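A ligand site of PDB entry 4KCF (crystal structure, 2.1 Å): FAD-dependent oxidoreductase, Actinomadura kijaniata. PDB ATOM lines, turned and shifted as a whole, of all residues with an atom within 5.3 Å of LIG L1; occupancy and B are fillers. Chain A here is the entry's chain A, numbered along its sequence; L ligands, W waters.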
ATOM      1  N   HIS A 118      11.659  21.252 -18.492  1.00  0.00           N
ATOM      2  CA  HIS A 118      12.285  20.263 -19.332  1.00  0.00           C
ATOM      3  C   HIS A 118      12.680  19.072 -18.456  1.00  0.00           C
ATOM      4  O   HIS A 118      12.567  17.932 -18.942  1.00  0.00           O
ATOM      5  CB  HIS A 118      13.525  20.777 -20.106  1.00  0.00           C
ATOM      6  CG  HIS A 118      14.460  19.666 -20.487  1.00  0.00           C
ATOM      7  ND1 HIS A 118      14.463  19.013 -21.706  1.00  0.00           N
ATOM      8  CD2 HIS A 118      15.442  19.084 -19.758  1.00  0.00           C
ATOM      9  CE1 HIS A 118      15.377  18.053 -21.697  1.00  0.00           C
ATOM     10  NE2 HIS A 118      15.986  18.076 -20.519  1.00  0.00           N
ATOM     11  N   MET A 119      13.163  19.296 -17.227  1.00  0.00           N
ATOM     12  CA  MET A 119      13.560  18.088 -16.467  1.00  0.00           C
ATOM     13  C   MET A 119      12.377  17.102 -16.278  1.00  0.00           C
ATOM     14  O   MET A 119      12.525  15.887 -16.433  1.00  0.00           O
ATOM     15  CB  MET A 119      14.192  18.415 -15.110  1.00  0.00           C
ATOM     16  CG  MET A 119      15.236  19.559 -15.047  1.00  0.00           C
ATOM     17  SD  MET A 119      16.627  19.069 -16.060  1.00  0.00           S
ATOM     18  CE  MET A 119      17.552  20.624 -15.932  1.00  0.00           C
ATOM     19  N   SER A 122      11.307  15.631 -19.990  1.00  0.00           N
ATOM     20  CA  SER A 122      12.328  14.652 -20.308  1.00  0.00           C
ATOM     21  C   SER A 122      12.032  13.353 -19.539  1.00  0.00           C
ATOM     22  O   SER A 122      12.094  12.291 -20.145  1.00  0.00           O
ATOM     23  CB  SER A 122      13.695  15.214 -19.907  1.00  0.00           C
ATOM     24  OG  SER A 122      14.671  14.169 -19.812  1.00  0.00           O
ATOM     25  N   ARG A 123      11.733  13.434 -18.249  1.00  0.00           N
ATOM     26  CA  ARG A 123      11.567  12.217 -17.421  1.00  0.00           C
ATOM     27  C   ARG A 123      10.366  11.370 -17.861  1.00  0.00           C
ATOM     28  O   ARG A 123      10.395  10.138 -17.852  1.00  0.00           O
ATOM     29  CB  ARG A 123      11.364  12.575 -15.949  1.00  0.00           C
ATOM     30  CG  ARG A 123      11.231  11.342 -15.039  1.00  0.00           C
ATOM     31  CD  ARG A 123      12.571  10.608 -15.001  1.00  0.00           C
ATOM     32  NE  ARG A 123      13.628  11.568 -14.687  1.00  0.00           N
ATOM     33  CZ  ARG A 123      14.926  11.306 -14.729  1.00  0.00           C
ATOM     34  NH1 ARG A 123      15.802  12.285 -14.438  1.00  0.00           N
ATOM     35  NH2 ARG A 123      15.342  10.089 -15.060  1.00  0.00           N
ATOM     36  N   LEU A 125       9.428  11.075 -20.856  1.00  0.00           N
ATOM     37  CA  LEU A 125       9.913  10.313 -21.999  1.00  0.00           C
ATOM     38  C   LEU A 125      10.795   9.127 -21.627  1.00  0.00           C
ATOM     39  O   LEU A 125      10.682   8.021 -22.175  1.00  0.00           O
ATOM     40  CB  LEU A 125      10.709  11.179 -23.025  1.00  0.00           C
ATOM     41  CG  LEU A 125       9.933  12.318 -23.673  1.00  0.00           C
ATOM     42  CD1 LEU A 125      10.894  13.200 -24.503  1.00  0.00           C
ATOM     43  CD2 LEU A 125       8.696  11.885 -24.509  1.00  0.00           C
ATOM     44  N   THR A 126      11.747   9.365 -20.748  1.00  0.00           N
ATOM     45  CA  THR A 126      12.713   8.322 -20.394  1.00  0.00           C
ATOM     46  C   THR A 126      12.095   7.224 -19.478  1.00  0.00           C
ATOM     47  O   THR A 126      12.479   6.049 -19.544  1.00  0.00           O
ATOM     48  CB  THR A 126      13.967   8.920 -19.705  1.00  0.00           C
ATOM     49  OG1 THR A 126      13.597   9.647 -18.531  1.00  0.00           O
ATOM     50  CG2 THR A 126      14.712   9.867 -20.681  1.00  0.00           C
ATOM     51  N   LEU A 127      11.223   7.641 -18.556  1.00  0.00           N
ATOM     52  CA  LEU A 127      10.456   6.700 -17.723  1.00  0.00           C
ATOM     53  C   LEU A 127       9.508   5.908 -18.631  1.00  0.00           C
ATOM     54  O   LEU A 127       9.435   4.692 -18.469  1.00  0.00           O
ATOM     55  CB  LEU A 127       9.734   7.394 -16.565  1.00  0.00           C
ATOM     56  CG  LEU A 127      10.638   7.642 -15.355  1.00  0.00           C
ATOM     57  CD1 LEU A 127       9.919   8.230 -14.174  1.00  0.00           C
ATOM     58  CD2 LEU A 127      11.545   6.489 -14.926  1.00  0.00           C
ATOM     59  N   TYR A 129      10.254   4.931 -21.547  1.00  0.00           N
ATOM     60  CA  TYR A 129      11.096   3.889 -22.112  1.00  0.00           C
ATOM     61  C   TYR A 129      11.321   2.771 -21.111  1.00  0.00           C
ATOM     62  O   TYR A 129      11.352   1.611 -21.522  1.00  0.00           O
ATOM     63  CB  TYR A 129      12.485   4.417 -22.508  1.00  0.00           C
ATOM     64  CG  TYR A 129      13.318   3.462 -23.337  1.00  0.00           C
ATOM     65  CD1 TYR A 129      13.166   3.460 -24.729  1.00  0.00           C
ATOM     66  CD2 TYR A 129      14.244   2.594 -22.760  1.00  0.00           C
ATOM     67  CE1 TYR A 129      13.926   2.626 -25.502  1.00  0.00           C
ATOM     68  CE2 TYR A 129      15.008   1.722 -23.534  1.00  0.00           C
ATOM     69  CZ  TYR A 129      14.831   1.762 -24.912  1.00  0.00           C
ATOM     70  OH  TYR A 129      15.514   0.975 -25.803  1.00  0.00           O
ATOM     71  N   GLU A 130      11.615   3.137 -19.856  1.00  0.00           N
ATOM     72  CA  GLU A 130      11.805   2.164 -18.778  1.00  0.00           C
ATOM     73  C   GLU A 130      10.531   1.286 -18.747  1.00  0.00           C
ATOM     74  O   GLU A 130      10.626   0.077 -18.815  1.00  0.00           O
ATOM     75  CB  GLU A 130      12.057   2.839 -17.427  1.00  0.00           C
ATOM     76  CG  GLU A 130      13.348   3.660 -17.329  1.00  0.00           C
ATOM     77  CD  GLU A 130      14.622   2.834 -17.355  1.00  0.00           C
ATOM     78  OE1 GLU A 130      15.740   3.379 -17.459  1.00  0.00           O
ATOM     79  OE2 GLU A 130      14.516   1.598 -17.268  1.00  0.00           O
ATOM     80  N   SER A 158      16.569  15.770 -11.193  1.00  0.00           N
ATOM     81  CA  SER A 158      17.609  14.920 -11.760  1.00  0.00           C
ATOM     82  C   SER A 158      18.915  15.398 -11.147  1.00  0.00           C
ATOM     83  O   SER A 158      19.192  16.606 -11.190  1.00  0.00           O
ATOM     84  CB  SER A 158      17.649  15.088 -13.273  1.00  0.00           C
ATOM     85  OG  SER A 158      18.904  14.562 -13.708  1.00  0.00           O
ATOM     86  N   ILE A 160      22.860  14.603 -11.394  1.00  0.00           N
ATOM     87  CA  ILE A 160      23.905  13.825 -12.062  1.00  0.00           C
ATOM     88  C   ILE A 160      25.305  14.113 -11.569  1.00  0.00           C
ATOM     89  O   ILE A 160      26.097  13.203 -11.336  1.00  0.00           O
ATOM     90  CB  ILE A 160      23.914  13.947 -13.622  1.00  0.00           C
ATOM     91  CG1 ILE A 160      22.591  13.472 -14.232  1.00  0.00           C
ATOM     92  CG2 ILE A 160      25.178  13.297 -14.215  1.00  0.00           C
ATOM     93  CD1 ILE A 160      22.222  11.992 -14.181  1.00  0.00           C
ATOM     94  N   VAL A 197      16.002  11.566  -9.219  1.00  0.00           N
ATOM     95  CA  VAL A 197      16.757  10.472  -9.842  1.00  0.00           C
ATOM     96  C   VAL A 197      18.252  10.806  -9.848  1.00  0.00           C
ATOM     97  O   VAL A 197      18.684  11.741 -10.531  1.00  0.00           O
ATOM     98  CB  VAL A 197      16.297  10.201 -11.283  1.00  0.00           C
ATOM     99  CG1 VAL A 197      17.190   9.139 -11.934  1.00  0.00           C
ATOM    100  CG2 VAL A 197      14.793   9.857 -11.312  1.00  0.00           C
ATOM    101  N   LEU A 255      17.384   1.856 -10.244  1.00  0.00           N
ATOM    102  CA  LEU A 255      17.680   1.468 -11.616  1.00  0.00           C
ATOM    103  C   LEU A 255      19.172   1.191 -11.862  1.00  0.00           C
ATOM    104  O   LEU A 255      19.983   2.114 -11.992  1.00  0.00           O
ATOM    105  CB  LEU A 255      17.162   2.544 -12.574  1.00  0.00           C
ATOM    106  CG  LEU A 255      15.656   2.837 -12.546  1.00  0.00           C
ATOM    107  CD1 LEU A 255      15.352   4.094 -13.365  1.00  0.00           C
ATOM    108  CD2 LEU A 255      14.817   1.686 -13.051  1.00  0.00           C
ATOM    109  N   ARG A 257      22.495   0.431 -13.767  1.00  0.00           N
ATOM    110  CA  ARG A 257      23.007   0.668 -15.122  1.00  0.00           C
ATOM    111  C   ARG A 257      24.143  -0.317 -15.403  1.00  0.00           C
ATOM    112  O   ARG A 257      24.119  -1.415 -14.860  1.00  0.00           O
ATOM    113  CB  ARG A 257      23.463   2.121 -15.275  1.00  0.00           C
ATOM    114  CG  ARG A 257      22.437   3.137 -14.846  1.00  0.00           C
ATOM    115  CD  ARG A 257      21.097   2.889 -15.508  1.00  0.00           C
ATOM    116  NE  ARG A 257      20.270   4.086 -15.321  1.00  0.00           N
ATOM    117  CZ  ARG A 257      18.996   4.195 -15.677  1.00  0.00           C
ATOM    118  NH1 ARG A 257      18.396   3.161 -16.262  1.00  0.00           N
ATOM    119  NH2 ARG A 257      18.343   5.333 -15.460  1.00  0.00           N
ATOM    120  N   ALA A 266      25.452   2.324 -26.936  1.00  0.00           N
ATOM    121  CA  ALA A 266      24.013   2.202 -26.907  1.00  0.00           C
ATOM    122  C   ALA A 266      23.423   3.129 -25.841  1.00  0.00           C
ATOM    123  O   ALA A 266      22.316   3.630 -26.044  1.00  0.00           O
ATOM    124  CB  ALA A 266      23.593   0.732 -26.681  1.00  0.00           C
ATOM    125  N   VAL A 267      24.126   3.400 -24.751  1.00  0.00           N
ATOM    126  CA  VAL A 267      23.641   4.346 -23.745  1.00  0.00           C
ATOM    127  C   VAL A 267      23.472   5.767 -24.268  1.00  0.00           C
ATOM    128  O   VAL A 267      22.783   6.566 -23.613  1.00  0.00           O
ATOM    129  CB  VAL A 267      24.514   4.475 -22.491  1.00  0.00           C
ATOM    130  CG1 VAL A 267      24.543   3.172 -21.742  1.00  0.00           C
ATOM    131  CG2 VAL A 267      25.927   4.951 -22.812  1.00  0.00           C
ATOM    132  N   ALA A 269      21.884   6.798 -26.721  1.00  0.00           N
ATOM    133  CA  ALA A 269      20.541   7.070 -27.183  1.00  0.00           C
ATOM    134  C   ALA A 269      19.749   7.658 -26.032  1.00  0.00           C
ATOM    135  O   ALA A 269      19.008   8.632 -26.258  1.00  0.00           O
ATOM    136  CB  ALA A 269      19.875   5.810 -27.650  1.00  0.00           C
ATOM    137  N   GLY A 270      19.925   7.096 -24.824  1.00  0.00           N
ATOM    138  CA  GLY A 270      19.117   7.548 -23.685  1.00  0.00           C
ATOM    139  C   GLY A 270      19.560   8.955 -23.295  1.00  0.00           C
ATOM    140  O   GLY A 270      18.758   9.852 -23.002  1.00  0.00           O
ATOM    141  N   GLN A 271      20.865   9.137 -23.358  1.00  0.00           N
ATOM    142  CA  GLN A 271      21.462  10.440 -23.082  1.00  0.00           C
ATOM    143  C   GLN A 271      21.150  11.500 -24.128  1.00  0.00           C
ATOM    144  O   GLN A 271      21.337  12.713 -23.869  1.00  0.00           O
ATOM    145  CB  GLN A 271      22.952  10.260 -22.886  1.00  0.00           C
ATOM    146  CG  GLN A 271      23.260   9.336 -21.693  1.00  0.00           C
ATOM    147  CD  GLN A 271      24.739   9.246 -21.488  1.00  0.00           C
ATOM    148  OE1 GLN A 271      25.476   9.815 -22.280  1.00  0.00           O
ATOM    149  NE2 GLN A 271      25.186   8.577 -20.432  1.00  0.00           N
ATOM    150  N   VAL A 273      17.885  11.287 -25.696  1.00  0.00           N
ATOM    151  CA  VAL A 273      16.479  11.473 -25.330  1.00  0.00           C
ATOM    152  C   VAL A 273      16.326  12.432 -24.158  1.00  0.00           C
ATOM    153  O   VAL A 273      15.445  13.282 -24.142  1.00  0.00           O
ATOM    154  CB  VAL A 273      15.704  10.130 -25.111  1.00  0.00           C
ATOM    155  CG1 VAL A 273      14.341  10.371 -24.508  1.00  0.00           C
ATOM    156  CG2 VAL A 273      15.394   9.494 -26.461  1.00  0.00           C
ATOM    157  N   SER A 274      17.146  12.243 -23.125  1.00  0.00           N
ATOM    158  CA  SER A 274      16.945  12.992 -21.908  1.00  0.00           C
ATOM    159  C   SER A 274      17.357  14.488 -21.911  1.00  0.00           C
ATOM    160  O   SER A 274      16.872  15.179 -21.019  1.00  0.00           O
ATOM    161  CB  SER A 274      17.651  12.288 -20.762  1.00  0.00           C
ATOM    162  OG  SER A 274      19.045  12.437 -20.914  1.00  0.00           O
ATOM    163  N   SER A 275      18.139  14.989 -22.880  1.00  0.00           N
ATOM    164  CA  SER A 275      18.518  16.415 -22.949  1.00  0.00           C
ATOM    165  C   SER A 275      18.241  17.119 -24.283  1.00  0.00           C
ATOM    166  O   SER A 275      18.144  18.324 -24.303  1.00  0.00           O
ATOM    167  CB  SER A 275      20.050  16.562 -22.902  1.00  0.00           C
ATOM    168  OG  SER A 275      20.418  16.419 -21.579  1.00  0.00           O
ATOM    169  N   LEU A 340      13.903   0.727 -33.140  1.00  0.00           N
ATOM    170  CA  LEU A 340      14.674  -0.175 -32.301  1.00  0.00           C
ATOM    171  C   LEU A 340      15.082  -1.434 -33.055  1.00  0.00           C
ATOM    172  O   LEU A 340      15.565  -2.382 -32.455  1.00  0.00           O
ATOM    173  CB  LEU A 340      13.862  -0.526 -31.066  1.00  0.00           C
ATOM    174  CG  LEU A 340      13.242   0.732 -30.465  1.00  0.00           C
ATOM    175  CD1 LEU A 340      11.909   0.447 -29.766  1.00  0.00           C
ATOM    176  CD2 LEU A 340      14.226   1.368 -29.499  1.00  0.00           C
ATOM    177  N   MET A 344      22.024  -1.236 -31.992  1.00  0.00           N
ATOM    178  CA  MET A 344      21.722  -0.314 -30.895  1.00  0.00           C
ATOM    179  C   MET A 344      22.901   0.592 -30.520  1.00  0.00           C
ATOM    180  O   MET A 344      22.735   1.708 -30.056  1.00  0.00           O
ATOM    181  CB  MET A 344      21.240  -1.079 -29.662  1.00  0.00           C
ATOM    182  CG  MET A 344      19.832  -1.684 -29.741  1.00  0.00           C
ATOM    183  SD  MET A 344      18.436  -0.572 -30.087  1.00  0.00           S
ATOM    184  CE  MET A 344      18.050   0.026 -28.454  1.00  0.00           C
ATOM    185  N   ARG A 347      22.763   3.185 -33.345  1.00  0.00           N
ATOM    186  CA  ARG A 347      21.630   4.054 -33.062  1.00  0.00           C
ATOM    187  C   ARG A 347      22.069   5.128 -32.056  1.00  0.00           C
ATOM    188  O   ARG A 347      21.758   6.317 -32.227  1.00  0.00           O
ATOM    189  CB  ARG A 347      20.451   3.221 -32.540  1.00  0.00           C
ATOM    190  CG  ARG A 347      19.310   4.006 -31.880  1.00  0.00           C
ATOM    191  CD  ARG A 347      18.137   3.090 -31.536  1.00  0.00           C
ATOM    192  NE  ARG A 347      17.044   3.778 -30.847  1.00  0.00           N
ATOM    193  CZ  ARG A 347      16.940   3.849 -29.508  1.00  0.00           C
ATOM    194  NH1 ARG A 347      15.885   4.472 -28.978  1.00  0.00           N
ATOM    195  NH2 ARG A 347      17.861   3.302 -28.702  1.00  0.00           N
ATOM    196  N   GLN A 402      25.920  19.279 -19.590  1.00  0.00           N
ATOM    197  CA  GLN A 402      26.421  18.009 -20.149  1.00  0.00           C
ATOM    198  C   GLN A 402      25.236  17.111 -20.474  1.00  0.00           C
ATOM    199  O   GLN A 402      24.248  17.166 -19.746  1.00  0.00           O
ATOM    200  CB  GLN A 402      27.215  17.252 -19.077  1.00  0.00           C
ATOM    201  CG  GLN A 402      28.466  18.034 -18.680  1.00  0.00           C
ATOM    202  CD  GLN A 402      29.610  17.857 -19.693  1.00  0.00           C
ATOM    203  OE1 GLN A 402      29.490  17.105 -20.667  1.00  0.00           O
ATOM    204  NE2 GLN A 402      30.721  18.552 -19.457  1.00  0.00           N
ATOM    205  N   PRO A 403      25.325  16.293 -21.536  1.00  0.00           N
ATOM    206  CA  PRO A 403      26.424  16.138 -22.495  1.00  0.00           C
ATOM    207  C   PRO A 403      26.275  17.119 -23.667  1.00  0.00           C
ATOM    208  O   PRO A 403      25.153  17.343 -24.117  1.00  0.00           O
ATOM    209  CB  PRO A 403      26.197  14.705 -23.033  1.00  0.00           C
ATOM    210  CG  PRO A 403      24.627  14.556 -23.029  1.00  0.00           C
ATOM    211  CD  PRO A 403      24.178  15.401 -21.824  1.00  0.00           C
ATOM    212  N   TYR A 426      29.820  10.142 -20.536  1.00  0.00           N
ATOM    213  CA  TYR A 426      30.350  11.167 -19.626  1.00  0.00           C
ATOM    214  C   TYR A 426      30.238  10.851 -18.124  1.00  0.00           C
ATOM    215  O   TYR A 426      31.090  11.247 -17.317  1.00  0.00           O
ATOM    216  CB  TYR A 426      29.722  12.534 -19.919  1.00  0.00           C
ATOM    217  CG  TYR A 426      28.291  12.763 -19.429  1.00  0.00           C
ATOM    218  CD1 TYR A 426      27.210  12.205 -20.099  1.00  0.00           C
ATOM    219  CD2 TYR A 426      28.030  13.545 -18.299  1.00  0.00           C
ATOM    220  CE1 TYR A 426      25.916  12.437 -19.642  1.00  0.00           C
ATOM    221  CE2 TYR A 426      26.736  13.787 -17.822  1.00  0.00           C
ATOM    222  CZ  TYR A 426      25.685  13.215 -18.510  1.00  0.00           C
ATOM    223  OH  TYR A 426      24.389  13.433 -18.106  1.00  0.00           O
ATOM    224  N   MET A 427      29.181  10.157 -17.711  1.00  0.00           N
ATOM    225  CA  MET A 427      29.041   9.705 -16.336  1.00  0.00           C
ATOM    226  C   MET A 427      30.044   8.599 -16.030  1.00  0.00           C
ATOM    227  O   MET A 427      30.590   8.528 -14.924  1.00  0.00           O
ATOM    228  CB  MET A 427      27.623   9.191 -16.086  1.00  0.00           C
ATOM    229  CG  MET A 427      26.564  10.179 -16.522  1.00  0.00           C
ATOM    230  SD  MET A 427      24.949   9.658 -15.922  1.00  0.00           S
ATOM    231  CE  MET A 427      23.932   9.900 -17.367  1.00  0.00           C
HETATM  232  O1  LIG L   1      20.514  10.797 -19.441  1.00  0.00           O
HETATM  233  P1  LIG L   1      20.331   9.448 -18.748  1.00  0.00           P
HETATM  234  O2  LIG L   1      21.539   8.575 -18.560  1.00  0.00           O
HETATM  235  O3  LIG L   1      19.741   9.671 -17.286  1.00  0.00           O
HETATM  236  P2  LIG L   1      18.599  10.684 -16.805  1.00  0.00           P
HETATM  237  O4  LIG L   1      18.166  10.115 -15.459  1.00  0.00           O
HETATM  238  O5  LIG L   1      19.376  12.049 -16.500  1.00  0.00           O
HETATM  239  C1  LIG L   1      19.315  13.228 -17.293  1.00  0.00           C
HETATM  240  C2  LIG L   1      20.489  14.151 -16.955  1.00  0.00           C
HETATM  241  C3  LIG L   1      20.218  15.557 -17.495  1.00  0.00           C
HETATM  242  C4  LIG L   1      20.565  15.411 -18.984  1.00  0.00           C
HETATM  243  N1  LIG L   1      21.131  16.543 -16.893  1.00  0.00           N
HETATM  244  C5  LIG L   1      18.815  16.084 -17.164  1.00  0.00           C
HETATM  245  O6  LIG L   1      18.785  16.682 -15.858  1.00  0.00           O
HETATM  246  O7  LIG L   1      18.483  17.171 -18.049  1.00  0.00           O
HETATM  247  C6  LIG L   1      17.724  15.064 -16.854  1.00  0.00           C
HETATM  248  C7  LIG L   1      16.274  15.323 -17.269  1.00  0.00           C
HETATM  249  O8  LIG L   1      18.004  13.675 -16.963  1.00  0.00           O
HETATM  250  O9  LIG L   1      17.491  10.983 -17.792  1.00  0.00           O
HETATM  251  O10 LIG L   1      19.245   8.633 -19.609  1.00  0.00           O
HETATM  252  C8  LIG L   1      18.950   7.302 -19.174  1.00  0.00           C
HETATM  253  C9  LIG L   1      17.488   7.134 -19.551  1.00  0.00           C
HETATM  254  C10 LIG L   1      16.877   5.818 -19.061  1.00  0.00           C
HETATM  255  O11 LIG L   1      16.151   6.091 -17.864  1.00  0.00           O
HETATM  256  C11 LIG L   1      15.907   5.388 -20.140  1.00  0.00           C
HETATM  257  C12 LIG L   1      16.193   6.312 -21.332  1.00  0.00           C
HETATM  258  O12 LIG L   1      17.366   7.073 -20.974  1.00  0.00           O
HETATM  259  N2  LIG L   1      16.421   5.664 -22.624  1.00  0.00           N
HETATM  260  C13 LIG L   1      15.664   6.031 -23.657  1.00  0.00           C
HETATM  261  O13 LIG L   1      14.672   6.935 -23.477  1.00  0.00           O
HETATM  262  N3  LIG L   1      15.809   5.513 -24.889  1.00  0.00           N
HETATM  263  C14 LIG L   1      16.791   4.613 -25.096  1.00  0.00           C
HETATM  264  O14 LIG L   1      16.998   4.065 -26.318  1.00  0.00           O
HETATM  265  C15 LIG L   1      17.682   4.206 -23.989  1.00  0.00           C
HETATM  266  C16 LIG L   1      18.780   3.211 -24.239  1.00  0.00           C
HETATM  267  C17 LIG L   1      17.427   4.778 -22.759  1.00  0.00           C
HETATM  268  N1  LG2 L   2      22.383  18.743 -14.189  1.00  0.00           N
HETATM  269  C1  LG2 L   2      21.531  17.781 -13.759  1.00  0.00           C
HETATM  270  O1  LG2 L   2      21.989  16.600 -13.728  1.00  0.00           O
HETATM  271  N2  LG2 L   2      20.249  18.081 -13.421  1.00  0.00           N
HETATM  272  C2  LG2 L   2      19.888  19.384 -13.449  1.00  0.00           C
HETATM  273  O2  LG2 L   2      18.621  19.726 -13.102  1.00  0.00           O
HETATM  274  C3  LG2 L   2      20.766  20.392 -13.932  1.00  0.00           C
HETATM  275  N3  LG2 L   2      20.415  21.715 -14.015  1.00  0.00           N
HETATM  276  C4  LG2 L   2      21.344  22.634 -14.403  1.00  0.00           C
HETATM  277  C5  LG2 L   2      20.962  23.977 -14.481  1.00  0.00           C
HETATM  278  C6  LG2 L   2      21.895  24.950 -14.901  1.00  0.00           C
HETATM  279  C7  LG2 L   2      21.487  26.400 -14.967  1.00  0.00           C
HETATM  280  C8  LG2 L   2      23.266  24.552 -15.271  1.00  0.00           C
HETATM  281  C9  LG2 L   2      24.327  25.526 -15.738  1.00  0.00           C
HETATM  282  C10 LG2 L   2      23.576  23.199 -15.188  1.00  0.00           C
HETATM  283  C11 LG2 L   2      22.637  22.234 -14.772  1.00  0.00           C
HETATM  284  N4  LG2 L   2      23.000  20.926 -14.676  1.00  0.00           N
HETATM  285  C12 LG2 L   2      22.054  20.029 -14.299  1.00  0.00           C
HETATM  286  C13 LG2 L   2      24.349  20.380 -14.937  1.00  0.00           C
HETATM  287  C14 LG2 L   2      25.239  20.509 -16.171  1.00  0.00           C
HETATM  288  O3  LG2 L   2      24.463  19.605 -16.965  1.00  0.00           O
HETATM  289  C15 LG2 L   2      26.773  20.248 -16.151  1.00  0.00           C
HETATM  290  O4  LG2 L   2      27.173  19.008 -15.515  1.00  0.00           O
HETATM  291  C16 LG2 L   2      27.822  21.263 -15.608  1.00  0.00           C
HETATM  292  O5  LG2 L   2      27.547  22.674 -15.381  1.00  0.00           O
HETATM  293  O   HOH W   1      14.081   8.040 -16.589  1.00  0.00           O
HETATM  294  O   HOH W   2      21.216  13.945 -21.630  1.00  0.00           O
HETATM  295  O   HOH W   3      19.211   7.723 -14.788  1.00  0.00           O
HETATM  296  O   HOH W   4      21.515  19.286 -17.623  1.00  0.00           O
HETATM  297  O   HOH W   5      14.017   5.874 -27.146  1.00  0.00           O
HETATM  298  O   HOH W   6      15.065  11.785 -18.057  1.00  0.00           O
HETATM  299  O   HOH W   7      23.968  15.733 -17.316  1.00  0.00           O
HETATM  300  O   HOH W   8      22.656  12.540 -19.854  1.00  0.00           O
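O14 of LIG L1 lies within hydrogen-bond range of NH2 of Arg 347, 2.6 Å away.
The side-chain hydroxyl of Ser 274 lies within hydrogen-bond range of an oxygen (O1) of LIG L1 (2.6 Å).
The side-chain carboxylate (OE1) of Glu 130 lies within hydrogen-bond range of an oxygen (O11) of LIG L1 (2.8 Å).
O4 of LIG L1 is in salt-bridge range of NH2 of Arg 123 (2.9 Å).
The side-chain hydroxyl (OG) of Ser 158 lies within hydrogen-bond range of an oxygen (O6) of LIG L1.
SD of Met 119 is in hydrogen-bond range of O6 of LIG L1, 3.2 Å away.
An oxygen (O11) of LIG L1 is in hydrogen-bond range of the guanidinium group (NH2) of Arg 257 (3.3 Å).
An oxygen (O14) of LIG L1 lies close to the side-chain hydroxyl (OH) of Tyr 129 (3.5 Å).
N2 of LG2 L2 sits at hydrogen-bond distance from O of Ser 158 (2.9 Å).
N of Ile 160 sits at hydrogen-bond distance from O1 of LG2 L2, 3.2 Å away.
An oxygen (O3) of LG2 L2 sits at hydrogen-bond distance from the backbone NH of Gln 402 (3.0 Å).
N2 of LG2 L2 lies within hydrogen-bond range of O6 of LIG L1.
The backbone carbonyl oxygen of Ser 274 lies within hydrogen-bond range of the side-chain hydroxyl of Ser 122, at 2.7 Å.
The side-chain hydroxyl (OG) of Ser 274 lies within hydrogen-bond range of the backbone carbonyl oxygen (O) of Gly 270, at 3.3 Å.
A ring nitrogen (NE2) of His 118 sits at hydrogen-bond distance from the backbone carbonyl oxygen (O) of Ser 274 (3.1 Å).
OE1 of Glu 130 is in salt-bridge range of NH1 of Arg 257 (2.9 Å).
O of Arg 123 lies within hydrogen-bond range of OG1 of Thr 126 (3.3 Å).
The backbone carbonyl oxygen (O) of Ser 122 sits at hydrogen-bond distance from the side-chain hydroxyl (OG1) of Thr 126, at 3.4 Å.
Residues that only touch LIG L1: Ser 275 (2.8 Å), Met 427 (3.0 Å), Ser 122 (3.2 Å), Gly 270 (3.3 Å), Ile 160 (3.5 Å), Thr 126 (3.5 Å), Val 273 (3.6 Å), Ala 269 (3.6 Å), His 118 (3.6 Å), Gln 271 (3.7 Å), Val 197 (3.8 Å) and Ala 266 (3.99 Å).
Hydrophobic or aromatic side chains that line LIG L1: His 118, Met 119, Tyr 129, Ile 160, Val 197, Ala 269, Val 273 and Met 427.
Of the 29 residues printed, 20 come within 4 Å of LIG L1.
Water W6 lies within hydrogen-bond range of an oxygen (O9) of LIG L1 (2.6 Å), the side-chain hydroxyl (OG1) of Thr 126 (2.6 Å), the side-chain hydroxyl (OG) of Ser 122 (3.0 Å) and the guanidinium group (NH2) of Arg 123 (3.5 Å).
Water W8 bridges the side-chain hydroxyl (OH) of Tyr 426 and an oxygen (O1) of LIG L1.
Water W4 bridges N1 of LIG L1 (2.9 Å) and O3 of LG2 L2 (3.0 Å).
Water W5 bridges N3 of LIG L1 and NH1 of Arg 347.
Water W7 lies within hydrogen-bond range of the side-chain hydroxyl of Tyr 426, the backbone carbonyl oxygen of Gln 402 and a nitrogen (N1) of LIG L1.
Water W2 lies within hydrogen-bond range of O of Gln 271 (2.6 Å), OG of Ser 275 (2.6 Å) and OG of Ser 274 (2.7 Å).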
